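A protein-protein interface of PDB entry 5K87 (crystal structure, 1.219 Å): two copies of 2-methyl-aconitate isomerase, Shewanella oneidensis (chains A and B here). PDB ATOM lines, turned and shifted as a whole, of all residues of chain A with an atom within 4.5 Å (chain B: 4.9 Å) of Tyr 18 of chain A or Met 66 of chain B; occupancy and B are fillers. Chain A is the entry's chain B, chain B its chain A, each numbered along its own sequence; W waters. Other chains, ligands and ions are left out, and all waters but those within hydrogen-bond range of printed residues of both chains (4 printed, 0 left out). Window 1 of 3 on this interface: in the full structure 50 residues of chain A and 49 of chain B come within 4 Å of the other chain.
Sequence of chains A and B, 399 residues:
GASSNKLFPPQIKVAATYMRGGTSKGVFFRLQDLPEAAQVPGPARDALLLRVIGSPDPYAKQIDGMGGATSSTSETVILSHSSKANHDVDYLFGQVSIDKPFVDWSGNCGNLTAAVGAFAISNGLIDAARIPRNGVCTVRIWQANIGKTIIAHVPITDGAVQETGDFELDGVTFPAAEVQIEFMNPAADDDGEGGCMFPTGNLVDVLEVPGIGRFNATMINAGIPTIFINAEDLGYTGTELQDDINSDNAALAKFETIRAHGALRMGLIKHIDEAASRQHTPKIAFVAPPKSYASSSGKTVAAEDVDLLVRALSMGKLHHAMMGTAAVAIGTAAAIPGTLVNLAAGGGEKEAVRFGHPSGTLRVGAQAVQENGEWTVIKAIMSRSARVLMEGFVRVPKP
NZ of Lys 25 of chain A lies within hydrogen-bond range of O of Gly 65 of chain B (2.9 Å).
NZ of Lys 25 of chain A lies within hydrogen-bond range of O of Gly 67 of chain B (2.9 Å).
Among the printed residues, pairs that only touch across the chains: Ala 16 of chain A with Met 390 of chain B (3.3 Å), Tyr 18 of chain A with Met 66 of chain B (3.6 Å), Tyr 18 of chain A with Met 390 of chain B (3.9 Å), Met 66 of chain A with Tyr 18 of chain B (3.7 Å), Met 66 of chain A with Met 390 of chain B (3.8 Å), Leu 389 of chain A with Gly 65 of chain B (3.8 Å), Leu 389 of chain A with Val 394 of chain B (3.3 Å), Met 390 of chain A with Tyr 18 of chain B (3.96 Å), Met 390 of chain A with Met 66 of chain B (3.7 Å), Met 390 of chain A with Met 390 of chain B (3.6 Å) and Met 390 of chain A with Val 394 of chain B (3.9 Å).
Tyr 18 of chain A touches Met 66 of chain B, and with the chains exchanged Met 66 of chain A touches Tyr 18 of chain B.
Tyr 18 of chain A touches Met 390 of chain B, and with the chains exchanged Met 390 of chain A touches Tyr 18 of chain B.
Met 66 of chain A touches Met 390 of chain B, and with the chains exchanged Met 390 of chain A touches Met 66 of chain B.
Met 390 of chain A touches its own counterpart, Met 390 of chain B.
Of the 13 pairs that touch across the chains among the printed residues, 7 have their exchanged pair printed and touching as well.
Hydrophobic or aromatic side chains of chain A within 4 Å of the printed part of chain B: Tyr 18, Met 66, Leu 389 and Met 390.
Hydrophobic or aromatic side chains of chain B that line the printed part of chain A: Tyr 18, Met 66, Met 390 and Val 394.
Among the printed residues, 13 pairs touch across the chains.
Among the printed residues, no Asp or Glu carboxylate lies within 4 Å of a Lys or Arg side-chain nitrogen of the other chain.
OH of Tyr 18 of chain A lies close to NZ of Lys 25 of chain A (3.2 Å).
The backbone NH of Tyr 18 of chain B lies within hydrogen-bond range of the backbone carbonyl oxygen of Met 390 of chain B, at 2.8 Å.
O of Tyr 18 of chain A sits at hydrogen-bond distance from N of Leu 389 of chain A (2.8 Å).
O of Ile 53 of chain B lies within hydrogen-bond range of N of Met 66 of chain B, 3.3 Å away.
The backbone carbonyl oxygen of Val 52 of chain B lies within hydrogen-bond range of the backbone NH of Met 66 of chain B (2.8 Å).
The backbone NH (N) of Gly 67 of chain B sits at hydrogen-bond distance from the backbone carbonyl oxygen (O) of Ile 53 of chain B, 2.9 Å away.
Tyr 18 of chain A touches two residues of chain B.
Gly 26 of chain A touches none of the printed residues of chain B.
Printed residues of chain B within 4 Å of Met 66 of chain A: Tyr 18 and Met 390.
Printed residues of chain B within 4 Å of Leu 389 of chain A: Gly 65 (3.8 Å) and Val 394 (3.3 Å).
Printed residues of chain B within 4 Å of Met 390 of chain A: Tyr 18 (3.96 Å), Met 66 (3.7 Å), Met 390 (3.6 Å) and Val 394 (3.9 Å).
Of the printed residues of chain A, Tyr 18 of chain B touches Met 66 (3.7 Å) and Met 390 (3.96 Å).
Printed residues of chain A within 4 Å of Met 66 of chain B: Tyr 18 (3.6 Å) and Met 390 (3.7 Å).
Thr 73 of chain B touches none of the printed residues of chain A.
Of the printed residues of chain A, Val 394 of chain B touches Leu 389 and Met 390.
The nearest residue of chain B that does not touch Tyr 18 of chain A is Gly 65 of chain B (4.4 Å).
The nearest residue of chain A that does not touch Met 66 of chain B is Leu 389 of chain A (4.04 Å).
Water W4 bridges OH of Tyr 18 of chain B (2.4 Å) and O of Met 66 of chain A (2.7 Å).
Water W1 lies within hydrogen-bond range of OH of Tyr 18 of chain A (2.5 Å), O of Met 66 of chain B (2.8 Å), NZ of Lys 25 of chain A (2.8 Å) and O of Gly 67 of chain B (3.5 Å).
Water W3 bridges the backbone carbonyl oxygen (O) of Gly 67 of chain B (2.9 Å) and the side-chain amino group (NZ) of Lys 25 of chain A (3.1 Å).
Water W2 lies within hydrogen-bond range of the side-chain amino group of Lys 25 of chain A (3.0 Å) and the backbone carbonyl oxygen of Gly 67 of chain B (3.5 Å).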
ATOM      1  N   ALA A  16      12.001  11.180  23.796  1.00  0.00           N
ATOM      2  CA  ALA A  16      10.621  10.726  23.807  1.00  0.00           C
ATOM      3  C   ALA A  16       9.762  11.612  22.927  1.00  0.00           C
ATOM      4  O   ALA A  16      10.110  12.750  22.612  1.00  0.00           O
ATOM      5  CB  ALA A  16      10.079  10.713  25.227  1.00  0.00           C
ATOM      6  N   THR A  17       8.618  11.066  22.537  1.00  0.00           N
ATOM      7  CA  THR A  17       7.630  11.817  21.777  1.00  0.00           C
ATOM      8  C   THR A  17       6.276  11.671  22.450  1.00  0.00           C
ATOM      9  O   THR A  17       5.855  10.566  22.765  1.00  0.00           O
ATOM     10  CB  THR A  17       7.538  11.294  20.335  1.00  0.00           C
ATOM     11  OG1 THR A  17       8.845  11.295  19.750  1.00  0.00           O
ATOM     12  CG2 THR A  17       6.628  12.169  19.504  1.00  0.00           C
ATOM     13  N   TYR A  18       5.608  12.799  22.683  1.00  0.00           N
ATOM     14  CA  TYR A  18       4.276  12.826  23.259  1.00  0.00           C
ATOM     15  C   TYR A  18       3.286  12.963  22.108  1.00  0.00           C
ATOM     16  O   TYR A  18       3.371  13.909  21.331  1.00  0.00           O
ATOM     17  CB  TYR A  18       4.203  14.031  24.188  1.00  0.00           C
ATOM     18  CG  TYR A  18       2.939  14.174  24.995  1.00  0.00           C
ATOM     19  CD1 TYR A  18       2.464  13.137  25.786  1.00  0.00           C
ATOM     20  CD2 TYR A  18       2.269  15.386  25.038  1.00  0.00           C
ATOM     21  CE1 TYR A  18       1.321  13.297  26.565  1.00  0.00           C
ATOM     22  CE2 TYR A  18       1.132  15.552  25.812  1.00  0.00           C
ATOM     23  CZ  TYR A  18       0.671  14.509  26.562  1.00  0.00           C
ATOM     24  OH  TYR A  18      -0.455  14.692  27.330  1.00  0.00           O
ATOM     25  N   MET A  19       2.382  11.994  21.973  1.00  0.00           N
ATOM     26  CA  MET A  19       1.487  11.935  20.813  1.00  0.00           C
ATOM     27  C   MET A  19       0.042  11.740  21.212  1.00  0.00           C
ATOM     28  O   MET A  19      -0.249  11.100  22.213  1.00  0.00           O
ATOM     29  CB  MET A  19       1.849  10.762  19.895  1.00  0.00           C
ATOM     30  CG  MET A  19       3.275  10.799  19.345  1.00  0.00           C
ATOM     31  SD  MET A  19       3.629   9.482  18.200  1.00  0.00           S
ATOM     32  CE  MET A  19       2.615   9.953  16.798  1.00  0.00           C
ATOM     33  N   LYS A  25      -3.780  10.033  24.677  1.00  0.00           N
ATOM     34  CA  LYS A  25      -2.447  10.642  24.608  1.00  0.00           C
ATOM     35  C   LYS A  25      -1.474   9.745  25.339  1.00  0.00           C
ATOM     36  O   LYS A  25      -1.787   9.226  26.412  1.00  0.00           O
ATOM     37  CB  LYS A  25      -2.411  12.023  25.279  1.00  0.00           C
ATOM     38  CG  LYS A  25      -3.232  13.077  24.563  1.00  0.00           C
ATOM     39  CD  LYS A  25      -2.969  14.476  25.114  1.00  0.00           C
ATOM     40  CE  LYS A  25      -3.553  14.731  26.488  1.00  0.00           C
ATOM     41  NZ  LYS A  25      -3.301  16.164  26.873  1.00  0.00           N
ATOM     42  N   GLY A  26      -0.277   9.586  24.784  1.00  0.00           N
ATOM     43  CA  GLY A  26       0.724   8.729  25.389  1.00  0.00           C
ATOM     44  C   GLY A  26       2.130   9.238  25.170  1.00  0.00           C
ATOM     45  O   GLY A  26       2.383  10.027  24.258  1.00  0.00           O
ATOM     46  N   VAL A  27       3.035   8.760  26.027  1.00  0.00           N
ATOM     47  CA  VAL A  27       4.454   9.033  25.870  1.00  0.00           C
ATOM     48  C   VAL A  27       5.112   7.831  25.197  1.00  0.00           C
ATOM     49  O   VAL A  27       5.001   6.708  25.690  1.00  0.00           O
ATOM     50  CB  VAL A  27       5.138   9.328  27.214  1.00  0.00           C
ATOM     51  CG1 VAL A  27       6.571   9.731  26.981  1.00  0.00           C
ATOM     52  CG2 VAL A  27       4.387  10.427  27.978  1.00  0.00           C
ATOM     53  N   MET A  66       3.915  13.661  33.049  1.00  0.00           N
ATOM     54  CA  MET A  66       3.284  13.829  31.747  1.00  0.00           C
ATOM     55  C   MET A  66       1.837  13.353  31.701  1.00  0.00           C
ATOM     56  O   MET A  66       1.139  13.623  30.717  1.00  0.00           O
ATOM     57  CB  MET A  66       4.069  13.066  30.686  1.00  0.00           C
ATOM     58  CG  MET A  66       5.496  13.548  30.474  1.00  0.00           C
ATOM     59  SD  MET A  66       5.601  15.270  29.978  1.00  0.00           S
ATOM     60  CE  MET A  66       4.727  15.232  28.408  1.00  0.00           C
ATOM     61  N   VAL A 388       1.853  14.147  16.474  1.00  0.00           N
ATOM     62  CA  VAL A 388       2.813  14.532  17.487  1.00  0.00           C
ATOM     63  C   VAL A 388       2.371  15.834  18.150  1.00  0.00           C
ATOM     64  O   VAL A 388       2.037  16.808  17.473  1.00  0.00           O
ATOM     65  CB  VAL A 388       4.219  14.700  16.864  1.00  0.00           C
ATOM     66  CG1 VAL A 388       5.178  15.288  17.888  1.00  0.00           C
ATOM     67  CG2 VAL A 388       4.731  13.354  16.312  1.00  0.00           C
ATOM     68  N   LEU A 389       2.384  15.839  19.483  1.00  0.00           N
ATOM     69  CA  LEU A 389       2.099  17.030  20.282  1.00  0.00           C
ATOM     70  C   LEU A 389       3.389  17.706  20.729  1.00  0.00           C
ATOM     71  O   LEU A 389       3.508  18.929  20.670  1.00  0.00           O
ATOM     72  CB  LEU A 389       1.281  16.640  21.510  1.00  0.00           C
ATOM     73  CG  LEU A 389       0.004  15.849  21.213  1.00  0.00           C
ATOM     74  CD1 LEU A 389      -0.716  15.496  22.485  1.00  0.00           C
ATOM     75  CD2 LEU A 389      -0.916  16.638  20.295  1.00  0.00           C
ATOM     76  N   MET A 390       4.358  16.915  21.176  1.00  0.00           N
ATOM     77  CA  MET A 390       5.653  17.446  21.597  1.00  0.00           C
ATOM     78  C   MET A 390       6.713  16.374  21.370  1.00  0.00           C
ATOM     79  O   MET A 390       6.460  15.182  21.556  1.00  0.00           O
ATOM     80  CB  MET A 390       5.631  17.874  23.063  1.00  0.00           C
ATOM     81  CG  MET A 390       6.844  18.692  23.508  1.00  0.00           C
ATOM     82  SD  MET A 390       6.633  19.442  25.129  1.00  0.00           S
ATOM     83  CE  MET A 390       8.097  20.484  25.165  1.00  0.00           C
ATOM     84  N   TYR B  18       7.888  22.193  28.735  1.00  0.00           N
ATOM     85  CA  TYR B  18       6.728  21.888  29.545  1.00  0.00           C
ATOM     86  C   TYR B  18       7.226  21.670  30.971  1.00  0.00           C
ATOM     87  O   TYR B  18       8.110  20.822  31.202  1.00  0.00           O
ATOM     88  CB  TYR B  18       6.083  20.636  28.967  1.00  0.00           C
ATOM     89  CG  TYR B  18       4.817  20.140  29.613  1.00  0.00           C
ATOM     90  CD1 TYR B  18       3.701  20.960  29.768  1.00  0.00           C
ATOM     91  CD2 TYR B  18       4.722  18.820  30.012  1.00  0.00           C
ATOM     92  CE1 TYR B  18       2.528  20.448  30.319  1.00  0.00           C
ATOM     93  CE2 TYR B  18       3.568  18.316  30.558  1.00  0.00           C
ATOM     94  CZ  TYR B  18       2.482  19.134  30.708  1.00  0.00           C
ATOM     95  OH  TYR B  18       1.345  18.585  31.255  1.00  0.00           O
ATOM     96  N   VAL B  27       3.097  25.350  29.532  1.00  0.00           N
ATOM     97  CA  VAL B  27       4.004  25.342  28.398  1.00  0.00           C
ATOM     98  C   VAL B  27       4.675  26.707  28.313  1.00  0.00           C
ATOM     99  O   VAL B  27       4.000  27.749  28.250  1.00  0.00           O
ATOM    100  CB  VAL B  27       3.270  25.022  27.076  1.00  0.00           C
ATOM    101  CG1 VAL B  27       4.277  24.930  25.946  1.00  0.00           C
ATOM    102  CG2 VAL B  27       2.463  23.735  27.195  1.00  0.00           C
ATOM    103  N   VAL B  52      -1.723  24.826  20.736  1.00  0.00           N
ATOM    104  CA  VAL B  52      -0.733  24.065  21.506  1.00  0.00           C
ATOM    105  C   VAL B  52      -1.413  23.345  22.676  1.00  0.00           C
ATOM    106  O   VAL B  52      -1.154  22.175  22.944  1.00  0.00           O
ATOM    107  CB  VAL B  52       0.406  24.961  22.029  1.00  0.00           C
ATOM    108  CG1 VAL B  52       1.254  24.219  23.058  1.00  0.00           C
ATOM    109  CG2 VAL B  52       1.270  25.460  20.867  1.00  0.00           C
ATOM    110  N   ILE B  53      -2.297  24.058  23.370  1.00  0.00           N
ATOM    111  CA  ILE B  53      -2.961  23.531  24.554  1.00  0.00           C
ATOM    112  C   ILE B  53      -4.100  22.547  24.221  1.00  0.00           C
ATOM    113  O   ILE B  53      -4.393  21.651  25.006  1.00  0.00           O
ATOM    114  CB  ILE B  53      -3.433  24.714  25.431  1.00  0.00           C
ATOM    115  CG1 ILE B  53      -2.237  25.396  26.094  1.00  0.00           C
ATOM    116  CG2 ILE B  53      -4.480  24.295  26.451  1.00  0.00           C
ATOM    117  CD1 ILE B  53      -1.532  24.536  27.153  1.00  0.00           C
ATOM    118  N   GLY B  54      -4.734  22.726  23.063  1.00  0.00           N
ATOM    119  CA  GLY B  54      -5.804  21.840  22.623  1.00  0.00           C
ATOM    120  C   GLY B  54      -7.190  22.450  22.773  1.00  0.00           C
ATOM    121  O   GLY B  54      -8.180  21.724  22.913  1.00  0.00           O
ATOM    122  N   ASP B  64      -6.278  16.660  22.410  1.00  0.00           N
ATOM    123  CA  ASP B  64      -5.584  17.045  21.187  1.00  0.00           C
ATOM    124  C   ASP B  64      -4.657  18.238  21.419  1.00  0.00           C
ATOM    125  O   ASP B  64      -4.475  19.071  20.543  1.00  0.00           O
ATOM    126  CB  ASP B  64      -6.597  17.339  20.084  1.00  0.00           C
ATOM    127  CG  ASP B  64      -6.056  17.096  18.695  1.00  0.00           C
ATOM    128  OD1 ASP B  64      -4.919  16.600  18.528  1.00  0.00           O
ATOM    129  OD2 ASP B  64      -6.849  17.377  17.757  1.00  0.00           O
ATOM    130  N   GLY B  65      -4.050  18.300  22.601  1.00  0.00           N
ATOM    131  CA  GLY B  65      -3.019  19.284  22.877  1.00  0.00           C
ATOM    132  C   GLY B  65      -2.315  19.006  24.188  1.00  0.00           C
ATOM    133  O   GLY B  65      -2.476  17.938  24.791  1.00  0.00           O
ATOM    134  N   MET B  66      -1.548  19.987  24.644  1.00  0.00           N
ATOM    135  CA  MET B  66      -0.741  19.826  25.842  1.00  0.00           C
ATOM    136  C   MET B  66      -1.499  20.058  27.140  1.00  0.00           C
ATOM    137  O   MET B  66      -0.973  19.776  28.218  1.00  0.00           O
ATOM    138  CB  MET B  66       0.423  20.810  25.808  1.00  0.00           C
ATOM    139  CG  MET B  66       1.387  20.584  24.671  1.00  0.00           C
ATOM    140  SD  MET B  66       2.180  18.973  24.682  1.00  0.00           S
ATOM    141  CE  MET B  66       3.086  19.002  26.225  1.00  0.00           C
ATOM    142  N   GLY B  67      -2.715  20.589  27.073  1.00  0.00           N
ATOM    143  CA  GLY B  67      -3.450  20.891  28.285  1.00  0.00           C
ATOM    144  C   GLY B  67      -3.932  19.641  28.991  1.00  0.00           C
ATOM    145  O   GLY B  67      -4.027  18.564  28.394  1.00  0.00           O
ATOM    146  N   GLY B  68      -4.261  19.798  30.269  1.00  0.00           N
ATOM    147  CA  GLY B  68      -4.732  18.694  31.083  1.00  0.00           C
ATOM    148  C   GLY B  68      -6.178  18.844  31.507  1.00  0.00           C
ATOM    149  O   GLY B  68      -6.638  18.146  32.416  1.00  0.00           O
ATOM    150  N   THR B  73      -3.763  23.282  34.566  1.00  0.00           N
ATOM    151  CA  THR B  73      -3.001  22.610  33.515  1.00  0.00           C
ATOM    152  C   THR B  73      -3.384  23.105  32.125  1.00  0.00           C
ATOM    153  O   THR B  73      -3.169  22.391  31.143  1.00  0.00           O
ATOM    154  CB  THR B  73      -3.177  21.075  33.548  1.00  0.00           C
ATOM    155  OG1 THR B  73      -4.552  20.739  33.328  1.00  0.00           O
ATOM    156  CG2 THR B  73      -2.722  20.495  34.873  1.00  0.00           C
ATOM    157  N   MET B 390       9.234  18.080  30.136  1.00  0.00           N
ATOM    158  CA  MET B 390       9.609  17.737  28.770  1.00  0.00           C
ATOM    159  C   MET B 390      10.133  18.991  28.096  1.00  0.00           C
ATOM    160  O   MET B 390       9.637  20.091  28.347  1.00  0.00           O
ATOM    161  CB  MET B 390       8.426  17.170  27.980  1.00  0.00           C
ATOM    162  CG  MET B 390       8.822  16.572  26.624  1.00  0.00           C
ATOM    163  SD  MET B 390       7.486  15.630  25.870  1.00  0.00           S
ATOM    164  CE  MET B 390       8.388  14.860  24.535  1.00  0.00           C
ATOM    165  N   VAL B 394       7.029  21.755  20.516  1.00  0.00           N
ATOM    166  CA  VAL B 394       5.612  21.453  20.340  1.00  0.00           C
ATOM    167  C   VAL B 394       5.244  21.644  18.875  1.00  0.00           C
ATOM    168  O   VAL B 394       5.910  22.383  18.138  1.00  0.00           O
ATOM    169  CB  VAL B 394       4.696  22.320  21.243  1.00  0.00           C
ATOM    170  CG1 VAL B 394       4.914  21.978  22.703  1.00  0.00           C
ATOM    171  CG2 VAL B 394       4.911  23.810  20.985  1.00  0.00           C
HETATM  172  O   HOH W   1      -0.931  17.012  28.088  1.00  0.00           O
HETATM  173  O   HOH W   2      -2.878  15.592  29.764  1.00  0.00           O
HETATM  174  O   HOH W   3      -5.651  16.174  28.829  1.00  0.00           O
HETATM  175  O   HOH W   4       0.667  16.301  30.905  1.00  0.00           O
